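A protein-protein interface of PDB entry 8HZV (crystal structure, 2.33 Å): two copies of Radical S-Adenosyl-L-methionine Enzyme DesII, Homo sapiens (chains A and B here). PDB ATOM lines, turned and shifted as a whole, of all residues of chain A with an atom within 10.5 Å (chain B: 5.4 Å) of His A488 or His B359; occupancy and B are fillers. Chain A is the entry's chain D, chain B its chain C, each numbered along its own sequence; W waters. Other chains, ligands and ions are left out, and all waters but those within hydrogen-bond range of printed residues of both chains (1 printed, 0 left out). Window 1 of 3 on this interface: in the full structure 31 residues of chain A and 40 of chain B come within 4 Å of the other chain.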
ATOM      1  N   GLY A  88     -13.779  -6.363 -27.024  1.00  0.00           N
ATOM      2  CA  GLY A  88     -13.374  -7.688 -26.603  1.00  0.00           C
ATOM      3  C   GLY A  88     -13.940  -8.825 -27.424  1.00  0.00           C
ATOM      4  O   GLY A  88     -13.573  -9.979 -27.183  1.00  0.00           O
ATOM      5  N   GLN A  89     -14.821  -8.536 -28.385  1.00  0.00           N
ATOM      6  CA  GLN A  89     -15.409  -9.543 -29.260  1.00  0.00           C
ATOM      7  C   GLN A  89     -14.778  -9.573 -30.643  1.00  0.00           C
ATOM      8  O   GLN A  89     -15.193 -10.380 -31.480  1.00  0.00           O
ATOM      9  CB  GLN A  89     -16.913  -9.304 -29.405  1.00  0.00           C
ATOM     10  CG  GLN A  89     -17.608  -8.973 -28.107  1.00  0.00           C
ATOM     11  CD  GLN A  89     -18.045 -10.212 -27.368  1.00  0.00           C
ATOM     12  OE1 GLN A  89     -19.222 -10.557 -27.367  1.00  0.00           O
ATOM     13  NE2 GLN A  89     -17.095 -10.897 -26.741  1.00  0.00           N
ATOM     14  N   VAL A  90     -13.806  -8.709 -30.913  1.00  0.00           N
ATOM     15  CA  VAL A  90     -13.164  -8.667 -32.222  1.00  0.00           C
ATOM     16  C   VAL A  90     -11.694  -9.017 -32.033  1.00  0.00           C
ATOM     17  O   VAL A  90     -10.872  -8.128 -31.764  1.00  0.00           O
ATOM     18  CB  VAL A  90     -13.346  -7.295 -32.893  1.00  0.00           C
ATOM     19  CG1 VAL A  90     -12.784  -7.313 -34.309  1.00  0.00           C
ATOM     20  CG2 VAL A  90     -14.816  -6.907 -32.907  1.00  0.00           C
ATOM     21  N   PRO A  91     -11.323 -10.293 -32.159  1.00  0.00           N
ATOM     22  CA  PRO A  91      -9.927 -10.681 -31.894  1.00  0.00           C
ATOM     23  C   PRO A  91      -8.923  -9.989 -32.792  1.00  0.00           C
ATOM     24  O   PRO A  91      -7.769  -9.802 -32.384  1.00  0.00           O
ATOM     25  CB  PRO A  91      -9.937 -12.200 -32.125  1.00  0.00           C
ATOM     26  CG  PRO A  91     -11.369 -12.607 -31.963  1.00  0.00           C
ATOM     27  CD  PRO A  91     -12.178 -11.451 -32.468  1.00  0.00           C
ATOM     28  N   ARG A  94      -7.674  -6.662 -31.044  1.00  0.00           N
ATOM     29  CA  ARG A  94      -6.684  -6.878 -29.994  1.00  0.00           C
ATOM     30  C   ARG A  94      -5.322  -7.199 -30.598  1.00  0.00           C
ATOM     31  O   ARG A  94      -4.291  -6.707 -30.123  1.00  0.00           O
ATOM     32  CB  ARG A  94      -7.139  -7.996 -29.052  1.00  0.00           C
ATOM     33  CG  ARG A  94      -6.019  -8.560 -28.184  1.00  0.00           C
ATOM     34  CD  ARG A  94      -6.549  -9.250 -26.934  1.00  0.00           C
ATOM     35  NE  ARG A  94      -5.525  -9.357 -25.897  1.00  0.00           N
ATOM     36  CZ  ARG A  94      -5.757  -9.206 -24.596  1.00  0.00           C
ATOM     37  NH1 ARG A  94      -6.981  -8.943 -24.166  1.00  0.00           N
ATOM     38  NH2 ARG A  94      -4.764  -9.317 -23.723  1.00  0.00           N
ATOM     39  N   GLU A  98      -1.766  -5.320 -29.971  1.00  0.00           N
ATOM     40  CA  GLU A  98      -0.595  -6.015 -29.444  1.00  0.00           C
ATOM     41  C   GLU A  98       0.543  -6.101 -30.451  1.00  0.00           C
ATOM     42  O   GLU A  98       1.697  -6.275 -30.046  1.00  0.00           O
ATOM     43  CB  GLU A  98      -0.975  -7.421 -28.977  1.00  0.00           C
ATOM     44  CG  GLU A  98      -1.708  -7.454 -27.648  1.00  0.00           C
ATOM     45  CD  GLU A  98      -1.984  -8.867 -27.168  1.00  0.00           C
ATOM     46  OE1 GLU A  98      -1.358  -9.806 -27.703  1.00  0.00           O
ATOM     47  OE2 GLU A  98      -2.831  -9.039 -26.262  1.00  0.00           O
ATOM     48  N   LEU A 111       1.543  -6.617 -20.466  1.00  0.00           N
ATOM     49  CA  LEU A 111       0.694  -7.797 -20.290  1.00  0.00           C
ATOM     50  C   LEU A 111       1.350  -8.868 -19.426  1.00  0.00           C
ATOM     51  O   LEU A 111       0.669  -9.409 -18.535  1.00  0.00           O
ATOM     52  CB  LEU A 111       0.270  -8.343 -21.657  1.00  0.00           C
ATOM     53  CG  LEU A 111      -0.574  -7.386 -22.503  1.00  0.00           C
ATOM     54  CD1 LEU A 111      -0.760  -7.927 -23.912  1.00  0.00           C
ATOM     55  CD2 LEU A 111      -1.920  -7.130 -21.841  1.00  0.00           C
ATOM     56  N   GLN A 115      -0.289 -10.112 -15.871  1.00  0.00           N
ATOM     57  CA  GLN A 115      -0.629 -11.509 -15.631  1.00  0.00           C
ATOM     58  C   GLN A 115      -0.128 -11.974 -14.267  1.00  0.00           C
ATOM     59  O   GLN A 115      -0.823 -12.709 -13.557  1.00  0.00           O
ATOM     60  CB  GLN A 115      -0.050 -12.380 -16.749  1.00  0.00           C
ATOM     61  CG  GLN A 115      -0.764 -13.703 -16.950  1.00  0.00           C
ATOM     62  CD  GLN A 115      -2.224 -13.530 -17.328  1.00  0.00           C
ATOM     63  OE1 GLN A 115      -2.582 -12.627 -18.088  1.00  0.00           O
ATOM     64  NE2 GLN A 115      -3.076 -14.394 -16.793  1.00  0.00           N
ATOM     65  N   ARG A 485      -5.485  -6.123 -20.382  1.00  0.00           N
ATOM     66  CA  ARG A 485      -4.899  -6.579 -19.129  1.00  0.00           C
ATOM     67  C   ARG A 485      -4.649  -8.082 -19.103  1.00  0.00           C
ATOM     68  O   ARG A 485      -3.496  -8.521 -19.148  1.00  0.00           O
ATOM     69  CB  ARG A 485      -5.794  -6.180 -17.954  1.00  0.00           C
ATOM     70  CG  ARG A 485      -5.189  -5.136 -17.041  1.00  0.00           C
ATOM     71  CD  ARG A 485      -5.658  -5.329 -15.610  1.00  0.00           C
ATOM     72  NE  ARG A 485      -7.116  -5.334 -15.514  1.00  0.00           N
ATOM     73  CZ  ARG A 485      -7.810  -6.132 -14.707  1.00  0.00           C
ATOM     74  NH1 ARG A 485      -9.136  -6.064 -14.683  1.00  0.00           N
ATOM     75  NH2 ARG A 485      -7.181  -6.999 -13.922  1.00  0.00           N
ATOM     76  N   LEU A 486      -5.709  -8.882 -19.028  1.00  0.00           N
ATOM     77  CA  LEU A 486      -5.585 -10.296 -18.706  1.00  0.00           C
ATOM     78  C   LEU A 486      -6.025 -11.177 -19.869  1.00  0.00           C
ATOM     79  O   LEU A 486      -6.564 -10.712 -20.877  1.00  0.00           O
ATOM     80  CB  LEU A 486      -6.405 -10.642 -17.456  1.00  0.00           C
ATOM     81  CG  LEU A 486      -6.002  -9.919 -16.169  1.00  0.00           C
ATOM     82  CD1 LEU A 486      -6.864 -10.381 -15.004  1.00  0.00           C
ATOM     83  CD2 LEU A 486      -4.523 -10.134 -15.870  1.00  0.00           C
ATOM     84  N   GLU A 487      -5.765 -12.477 -19.704  1.00  0.00           N
ATOM     85  CA  GLU A 487      -6.264 -13.528 -20.583  1.00  0.00           C
ATOM     86  C   GLU A 487      -6.904 -14.626 -19.737  1.00  0.00           C
ATOM     87  O   GLU A 487      -7.027 -14.478 -18.517  1.00  0.00           O
ATOM     88  CB  GLU A 487      -5.138 -14.093 -21.449  1.00  0.00           C
ATOM     89  CG  GLU A 487      -4.613 -13.120 -22.491  1.00  0.00           C
ATOM     90  CD  GLU A 487      -4.898 -13.577 -23.907  1.00  0.00           C
ATOM     91  OE1 GLU A 487      -5.969 -13.222 -24.445  1.00  0.00           O
ATOM     92  OE2 GLU A 487      -4.053 -14.295 -24.481  1.00  0.00           O
ATOM     93  N   HIS A 488      -7.311 -15.730 -20.361  1.00  0.00           N
ATOM     94  CA  HIS A 488      -8.013 -16.812 -19.673  1.00  0.00           C
ATOM     95  C   HIS A 488      -7.110 -18.039 -19.633  1.00  0.00           C
ATOM     96  O   HIS A 488      -6.871 -18.675 -20.665  1.00  0.00           O
ATOM     97  CB  HIS A 488      -9.342 -17.113 -20.362  1.00  0.00           C
ATOM     98  CG  HIS A 488     -10.295 -15.958 -20.352  1.00  0.00           C
ATOM     99  ND1 HIS A 488     -10.541 -15.182 -21.464  1.00  0.00           N
ATOM    100  CD2 HIS A 488     -11.046 -15.432 -19.355  1.00  0.00           C
ATOM    101  CE1 HIS A 488     -11.408 -14.234 -21.156  1.00  0.00           C
ATOM    102  NE2 HIS A 488     -11.731 -14.363 -19.882  1.00  0.00           N
ATOM    103  N   HIS A 489      -6.613 -18.369 -18.439  1.00  0.00           N
ATOM    104  CA  HIS A 489      -5.684 -19.477 -18.233  1.00  0.00           C
ATOM    105  C   HIS A 489      -6.337 -20.496 -17.308  1.00  0.00           C
ATOM    106  O   HIS A 489      -6.590 -20.204 -16.132  1.00  0.00           O
ATOM    107  CB  HIS A 489      -4.356 -18.976 -17.656  1.00  0.00           C
ATOM    108  CG  HIS A 489      -3.633 -19.994 -16.824  1.00  0.00           C
ATOM    109  ND1 HIS A 489      -3.263 -21.230 -17.314  1.00  0.00           N
ATOM    110  CD2 HIS A 489      -3.215 -19.960 -15.536  1.00  0.00           C
ATOM    111  CE1 HIS A 489      -2.649 -21.912 -16.363  1.00  0.00           C
ATOM    112  NE2 HIS A 489      -2.607 -21.164 -15.275  1.00  0.00           N
ATOM    113  N   HIS A 490      -6.619 -21.695 -17.848  1.00  0.00           N
ATOM    114  CA  HIS A 490      -7.211 -22.778 -17.063  1.00  0.00           C
ATOM    115  C   HIS A 490      -6.734 -24.151 -17.534  1.00  0.00           C
ATOM    116  O   HIS A 490      -7.474 -25.135 -17.412  1.00  0.00           O
ATOM    117  CB  HIS A 490      -8.753 -22.750 -17.125  1.00  0.00           C
ATOM    118  CG  HIS A 490      -9.362 -21.440 -16.721  1.00  0.00           C
ATOM    119  ND1 HIS A 490      -9.734 -21.157 -15.423  1.00  0.00           N
ATOM    120  CD2 HIS A 490      -9.672 -20.340 -17.449  1.00  0.00           C
ATOM    121  CE1 HIS A 490     -10.240 -19.937 -15.367  1.00  0.00           C
ATOM    122  NE2 HIS A 490     -10.213 -19.419 -16.582  1.00  0.00           N
ATOM    123  N   HIS A 491      -5.514 -24.242 -18.065  1.00  0.00           N
ATOM    124  CA  HIS A 491      -5.071 -25.487 -18.690  1.00  0.00           C
ATOM    125  C   HIS A 491      -4.646 -26.552 -17.688  1.00  0.00           C
ATOM    126  O   HIS A 491      -4.649 -27.738 -18.032  1.00  0.00           O
ATOM    127  CB  HIS A 491      -3.926 -25.203 -19.664  1.00  0.00           C
ATOM    128  CG  HIS A 491      -4.026 -23.863 -20.320  1.00  0.00           C
ATOM    129  ND1 HIS A 491      -4.942 -23.589 -21.314  1.00  0.00           N
ATOM    130  CD2 HIS A 491      -3.338 -22.715 -20.116  1.00  0.00           C
ATOM    131  CE1 HIS A 491      -4.812 -22.331 -21.695  1.00  0.00           C
ATOM    132  NE2 HIS A 491      -3.843 -21.780 -20.985  1.00  0.00           N
ATOM    133  N   HIS A 492      -4.291 -26.168 -16.466  1.00  0.00           N
ATOM    134  CA  HIS A 492      -4.132 -27.135 -15.390  1.00  0.00           C
ATOM    135  C   HIS A 492      -5.437 -27.377 -14.641  1.00  0.00           C
ATOM    136  O   HIS A 492      -5.450 -28.165 -13.688  1.00  0.00           O
ATOM    137  CB  HIS A 492      -3.042 -26.679 -14.406  1.00  0.00           C
ATOM    138  CG  HIS A 492      -1.817 -26.110 -15.063  1.00  0.00           C
ATOM    139  ND1 HIS A 492      -1.335 -26.564 -16.274  1.00  0.00           N
ATOM    140  CD2 HIS A 492      -0.966 -25.133 -14.665  1.00  0.00           C
ATOM    141  CE1 HIS A 492      -0.249 -25.884 -16.598  1.00  0.00           C
ATOM    142  NE2 HIS A 492      -0.003 -25.010 -15.639  1.00  0.00           N
ATOM    143  N   HIS A 493      -6.519 -26.717 -15.062  1.00  0.00           N
ATOM    144  CA  HIS A 493      -7.844 -26.774 -14.430  1.00  0.00           C
ATOM    145  C   HIS A 493      -7.788 -26.718 -12.907  1.00  0.00           C
ATOM    146  O   HIS A 493      -8.316 -27.600 -12.230  1.00  0.00           O
ATOM    147  CB  HIS A 493      -8.603 -28.032 -14.867  1.00  0.00           C
ATOM    148  CG  HIS A 493      -8.428 -28.378 -16.313  1.00  0.00           C
ATOM    149  ND1 HIS A 493      -7.241 -28.855 -16.829  1.00  0.00           N
ATOM    150  CD2 HIS A 493      -9.294 -28.323 -17.354  1.00  0.00           C
ATOM    151  CE1 HIS A 493      -7.383 -29.074 -18.123  1.00  0.00           C
ATOM    152  NE2 HIS A 493      -8.619 -28.758 -18.466  1.00  0.00           N
ATOM    153  N   HIS B 235     -12.429 -14.613  -9.824  1.00  0.00           N
ATOM    154  CA  HIS B 235     -11.946 -14.279 -11.157  1.00  0.00           C
ATOM    155  C   HIS B 235     -12.836 -14.892 -12.229  1.00  0.00           C
ATOM    156  O   HIS B 235     -13.145 -14.244 -13.236  1.00  0.00           O
ATOM    157  CB  HIS B 235     -10.505 -14.745 -11.338  1.00  0.00           C
ATOM    158  CG  HIS B 235      -9.934 -14.404 -12.679  1.00  0.00           C
ATOM    159  ND1 HIS B 235      -9.818 -15.326 -13.698  1.00  0.00           N
ATOM    160  CD2 HIS B 235      -9.466 -13.233 -13.176  1.00  0.00           C
ATOM    161  CE1 HIS B 235      -9.292 -14.742 -14.759  1.00  0.00           C
ATOM    162  NE2 HIS B 235      -9.070 -13.472 -14.470  1.00  0.00           N
ATOM    163  N   ASN B 281     -15.513 -13.587 -14.912  1.00  0.00           N
ATOM    164  CA  ASN B 281     -15.513 -14.326 -16.163  1.00  0.00           C
ATOM    165  C   ASN B 281     -16.326 -15.603 -16.009  1.00  0.00           C
ATOM    166  O   ASN B 281     -16.486 -16.134 -14.907  1.00  0.00           O
ATOM    167  CB  ASN B 281     -14.085 -14.660 -16.602  1.00  0.00           C
ATOM    168  CG  ASN B 281     -13.247 -13.420 -16.843  1.00  0.00           C
ATOM    169  OD1 ASN B 281     -13.717 -12.441 -17.422  1.00  0.00           O
ATOM    170  ND2 ASN B 281     -11.998 -13.454 -16.394  1.00  0.00           N
ATOM    171  N   ASP B 316     -16.907 -16.173 -21.894  1.00  0.00           N
ATOM    172  CA  ASP B 316     -15.527 -15.759 -22.112  1.00  0.00           C
ATOM    173  C   ASP B 316     -14.654 -16.853 -22.720  1.00  0.00           C
ATOM    174  O   ASP B 316     -13.798 -16.551 -23.557  1.00  0.00           O
ATOM    175  CB  ASP B 316     -14.924 -15.271 -20.794  1.00  0.00           C
ATOM    176  CG  ASP B 316     -15.706 -14.116 -20.193  1.00  0.00           C
ATOM    177  OD1 ASP B 316     -16.623 -14.368 -19.380  1.00  0.00           O
ATOM    178  OD2 ASP B 316     -15.412 -12.955 -20.544  1.00  0.00           O
ATOM    179  N   PHE B 317     -14.841 -18.116 -22.332  1.00  0.00           N
ATOM    180  CA  PHE B 317     -13.967 -19.162 -22.846  1.00  0.00           C
ATOM    181  C   PHE B 317     -14.665 -20.514 -22.791  1.00  0.00           C
ATOM    182  O   PHE B 317     -15.684 -20.684 -22.117  1.00  0.00           O
ATOM    183  CB  PHE B 317     -12.640 -19.214 -22.075  1.00  0.00           C
ATOM    184  CG  PHE B 317     -12.778 -19.653 -20.644  1.00  0.00           C
ATOM    185  CD1 PHE B 317     -12.669 -20.992 -20.300  1.00  0.00           C
ATOM    186  CD2 PHE B 317     -13.001 -18.726 -19.639  1.00  0.00           C
ATOM    187  CE1 PHE B 317     -12.791 -21.400 -18.979  1.00  0.00           C
ATOM    188  CE2 PHE B 317     -13.123 -19.125 -18.319  1.00  0.00           C
ATOM    189  CZ  PHE B 317     -13.019 -20.464 -17.988  1.00  0.00           C
ATOM    190  N   VAL B 318     -14.092 -21.473 -23.515  1.00  0.00           N
ATOM    191  CA  VAL B 318     -14.520 -22.868 -23.489  1.00  0.00           C
ATOM    192  C   VAL B 318     -13.280 -23.746 -23.585  1.00  0.00           C
ATOM    193  O   VAL B 318     -12.421 -23.517 -24.445  1.00  0.00           O
ATOM    194  CB  VAL B 318     -15.503 -23.199 -24.632  1.00  0.00           C
ATOM    195  CG1 VAL B 318     -15.599 -24.698 -24.828  1.00  0.00           C
ATOM    196  CG2 VAL B 318     -16.884 -22.620 -24.345  1.00  0.00           C
ATOM    197  N   GLY B 357     -15.892 -13.538 -29.857  1.00  0.00           N
ATOM    198  CA  GLY B 357     -15.049 -13.292 -28.706  1.00  0.00           C
ATOM    199  C   GLY B 357     -14.734 -14.506 -27.869  1.00  0.00           C
ATOM    200  O   GLY B 357     -13.886 -14.428 -26.976  1.00  0.00           O
ATOM    201  N   LEU B 358     -15.389 -15.633 -28.135  1.00  0.00           N
ATOM    202  CA  LEU B 358     -15.216 -16.829 -27.320  1.00  0.00           C
ATOM    203  C   LEU B 358     -13.812 -17.394 -27.500  1.00  0.00           C
ATOM    204  O   LEU B 358     -13.421 -17.764 -28.613  1.00  0.00           O
ATOM    205  CB  LEU B 358     -16.262 -17.874 -27.695  1.00  0.00           C
ATOM    206  CG  LEU B 358     -16.082 -19.257 -27.070  1.00  0.00           C
ATOM    207  CD1 LEU B 358     -16.466 -19.212 -25.600  1.00  0.00           C
ATOM    208  CD2 LEU B 358     -16.906 -20.296 -27.811  1.00  0.00           C
ATOM    209  N   HIS B 359     -13.055 -17.466 -26.409  1.00  0.00           N
ATOM    210  CA  HIS B 359     -11.740 -18.090 -26.445  1.00  0.00           C
ATOM    211  C   HIS B 359     -11.884 -19.609 -26.423  1.00  0.00           C
ATOM    212  O   HIS B 359     -12.657 -20.157 -25.633  1.00  0.00           O
ATOM    213  CB  HIS B 359     -10.890 -17.621 -25.266  1.00  0.00           C
ATOM    214  CG  HIS B 359      -9.565 -18.311 -25.170  1.00  0.00           C
ATOM    215  ND1 HIS B 359      -9.233 -19.144 -24.123  1.00  0.00           N
ATOM    216  CD2 HIS B 359      -8.494 -18.300 -25.997  1.00  0.00           C
ATOM    217  CE1 HIS B 359      -8.012 -19.612 -24.307  1.00  0.00           C
ATOM    218  NE2 HIS B 359      -7.542 -19.115 -25.436  1.00  0.00           N
ATOM    219  N   ILE B 360     -11.140 -20.284 -27.297  1.00  0.00           N
ATOM    220  CA  ILE B 360     -11.139 -21.738 -27.391  1.00  0.00           C
ATOM    221  C   ILE B 360      -9.733 -22.241 -27.108  1.00  0.00           C
ATOM    222  O   ILE B 360      -8.749 -21.620 -27.523  1.00  0.00           O
ATOM    223  CB  ILE B 360     -11.606 -22.230 -28.777  1.00  0.00           C
ATOM    224  CG1 ILE B 360     -12.918 -21.563 -29.182  1.00  0.00           C
ATOM    225  CG2 ILE B 360     -11.752 -23.747 -28.792  1.00  0.00           C
ATOM    226  CD1 ILE B 360     -13.275 -21.818 -30.628  1.00  0.00           C
ATOM    227  N   ASP B 361      -9.643 -23.363 -26.401  1.00  0.00           N
ATOM    228  CA  ASP B 361      -8.384 -24.077 -26.257  1.00  0.00           C
ATOM    229  C   ASP B 361      -8.690 -25.564 -26.154  1.00  0.00           C
ATOM    230  O   ASP B 361      -9.777 -25.962 -25.727  1.00  0.00           O
ATOM    231  CB  ASP B 361      -7.582 -23.589 -25.044  1.00  0.00           C
ATOM    232  CG  ASP B 361      -8.109 -24.138 -23.740  1.00  0.00           C
ATOM    233  OD1 ASP B 361      -9.343 -24.151 -23.559  1.00  0.00           O
ATOM    234  OD2 ASP B 361      -7.289 -24.559 -22.897  1.00  0.00           O
HETATM  235  O   HOH W   1     -18.581 -13.456 -28.692  1.00  0.00           O
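OD2 of Asp B361 lies within hydrogen-bond range of ND1 of His A491 (3.0 Å).
The backbone carbonyl oxygen (O) of His B235 sits at hydrogen-bond distance from the backbone NH (N) of Asn B281 (3.0 Å). The backbone carbonyl oxygen (O) of Asp B316 is in hydrogen-bond range of the backbone NH (N) of His B359 (3.1 Å). N of Val B318 is in hydrogen-bond range of O of His B359. The backbone carbonyl oxygen (O) of Val B318 is in hydrogen-bond range of the backbone NH (N) of Asp B361 (3.4 Å). The backbone carbonyl oxygen of His A491 lies close to a ring nitrogen (ND1) of His A493.
Gly A88 touches Gly B357 (O to CA, 3.9 Å). O of Gln A89 touches N of Gly B357, at 3.6 Å. His B235 touches Leu A486 (NE2 to CD1, 3.8 Å). NE2 of His A488 touches CG of Asn B281, 3.5 Å away. NE2 of His A488 touches CB of Asp B316, 3.4 Å away. His A488 touches Phe B317. O of His A488 touches CE1 of His B359 (3.9 Å). Phe B317 touches His A490 (CZ to NE2, 3.3 Å).
Printed residues of chain B within 4 Å of Gly A88: Gly B357 (3.9 Å). Arg A485 touches none of the printed residues of chain B. His A488 touches four residues of chain B. His A489 touches none of the printed residues of chain B. Asp B316 touches just one residue of chain A: His A488. Phe B317 touches just these residues of chain A: His A488 and His A490. No residue of chain A comes within 4 Å of Val B318. No residue of chain A comes within 4 Å of Leu B358. His B359 touches just one residue of chain A: His A488. No residue of chain A comes within 4 Å of Ile B360. Of the printed residues of chain A, Asp B361 touches His A491. The nearest residue of chain A that does not touch His B359 is His A491 (4.9 Å). The nearest printed residue of chain B that does not touch Leu A486 is Asn B281 (6.1 Å).
Of the 10 printed residues of chain B, 7 touch a printed residue of chain A. Hydrophobic or aromatic side chains of chain B within 4 Å of the printed part of chain A: His B235, Phe B317 and His B359. Hydrophobic or aromatic side chains of chain A that line the printed part of chain B: Leu A486, His A488, His A490 and His A491. Among the printed residues, no Asp or Glu carboxylate lies within 4 Å of a Lys or Arg side-chain nitrogen of the other chain.
No position is printed for both chains. Of the 9 pairs that touch across the chains among the printed residues, none has its exchanged pair printed and touching as well.
Water W1 bridges the backbone NH (N) of Gly B357 (2.9 Å) and the side-chain amide oxygen (OE1) of Gln A89 (3.3 Å).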
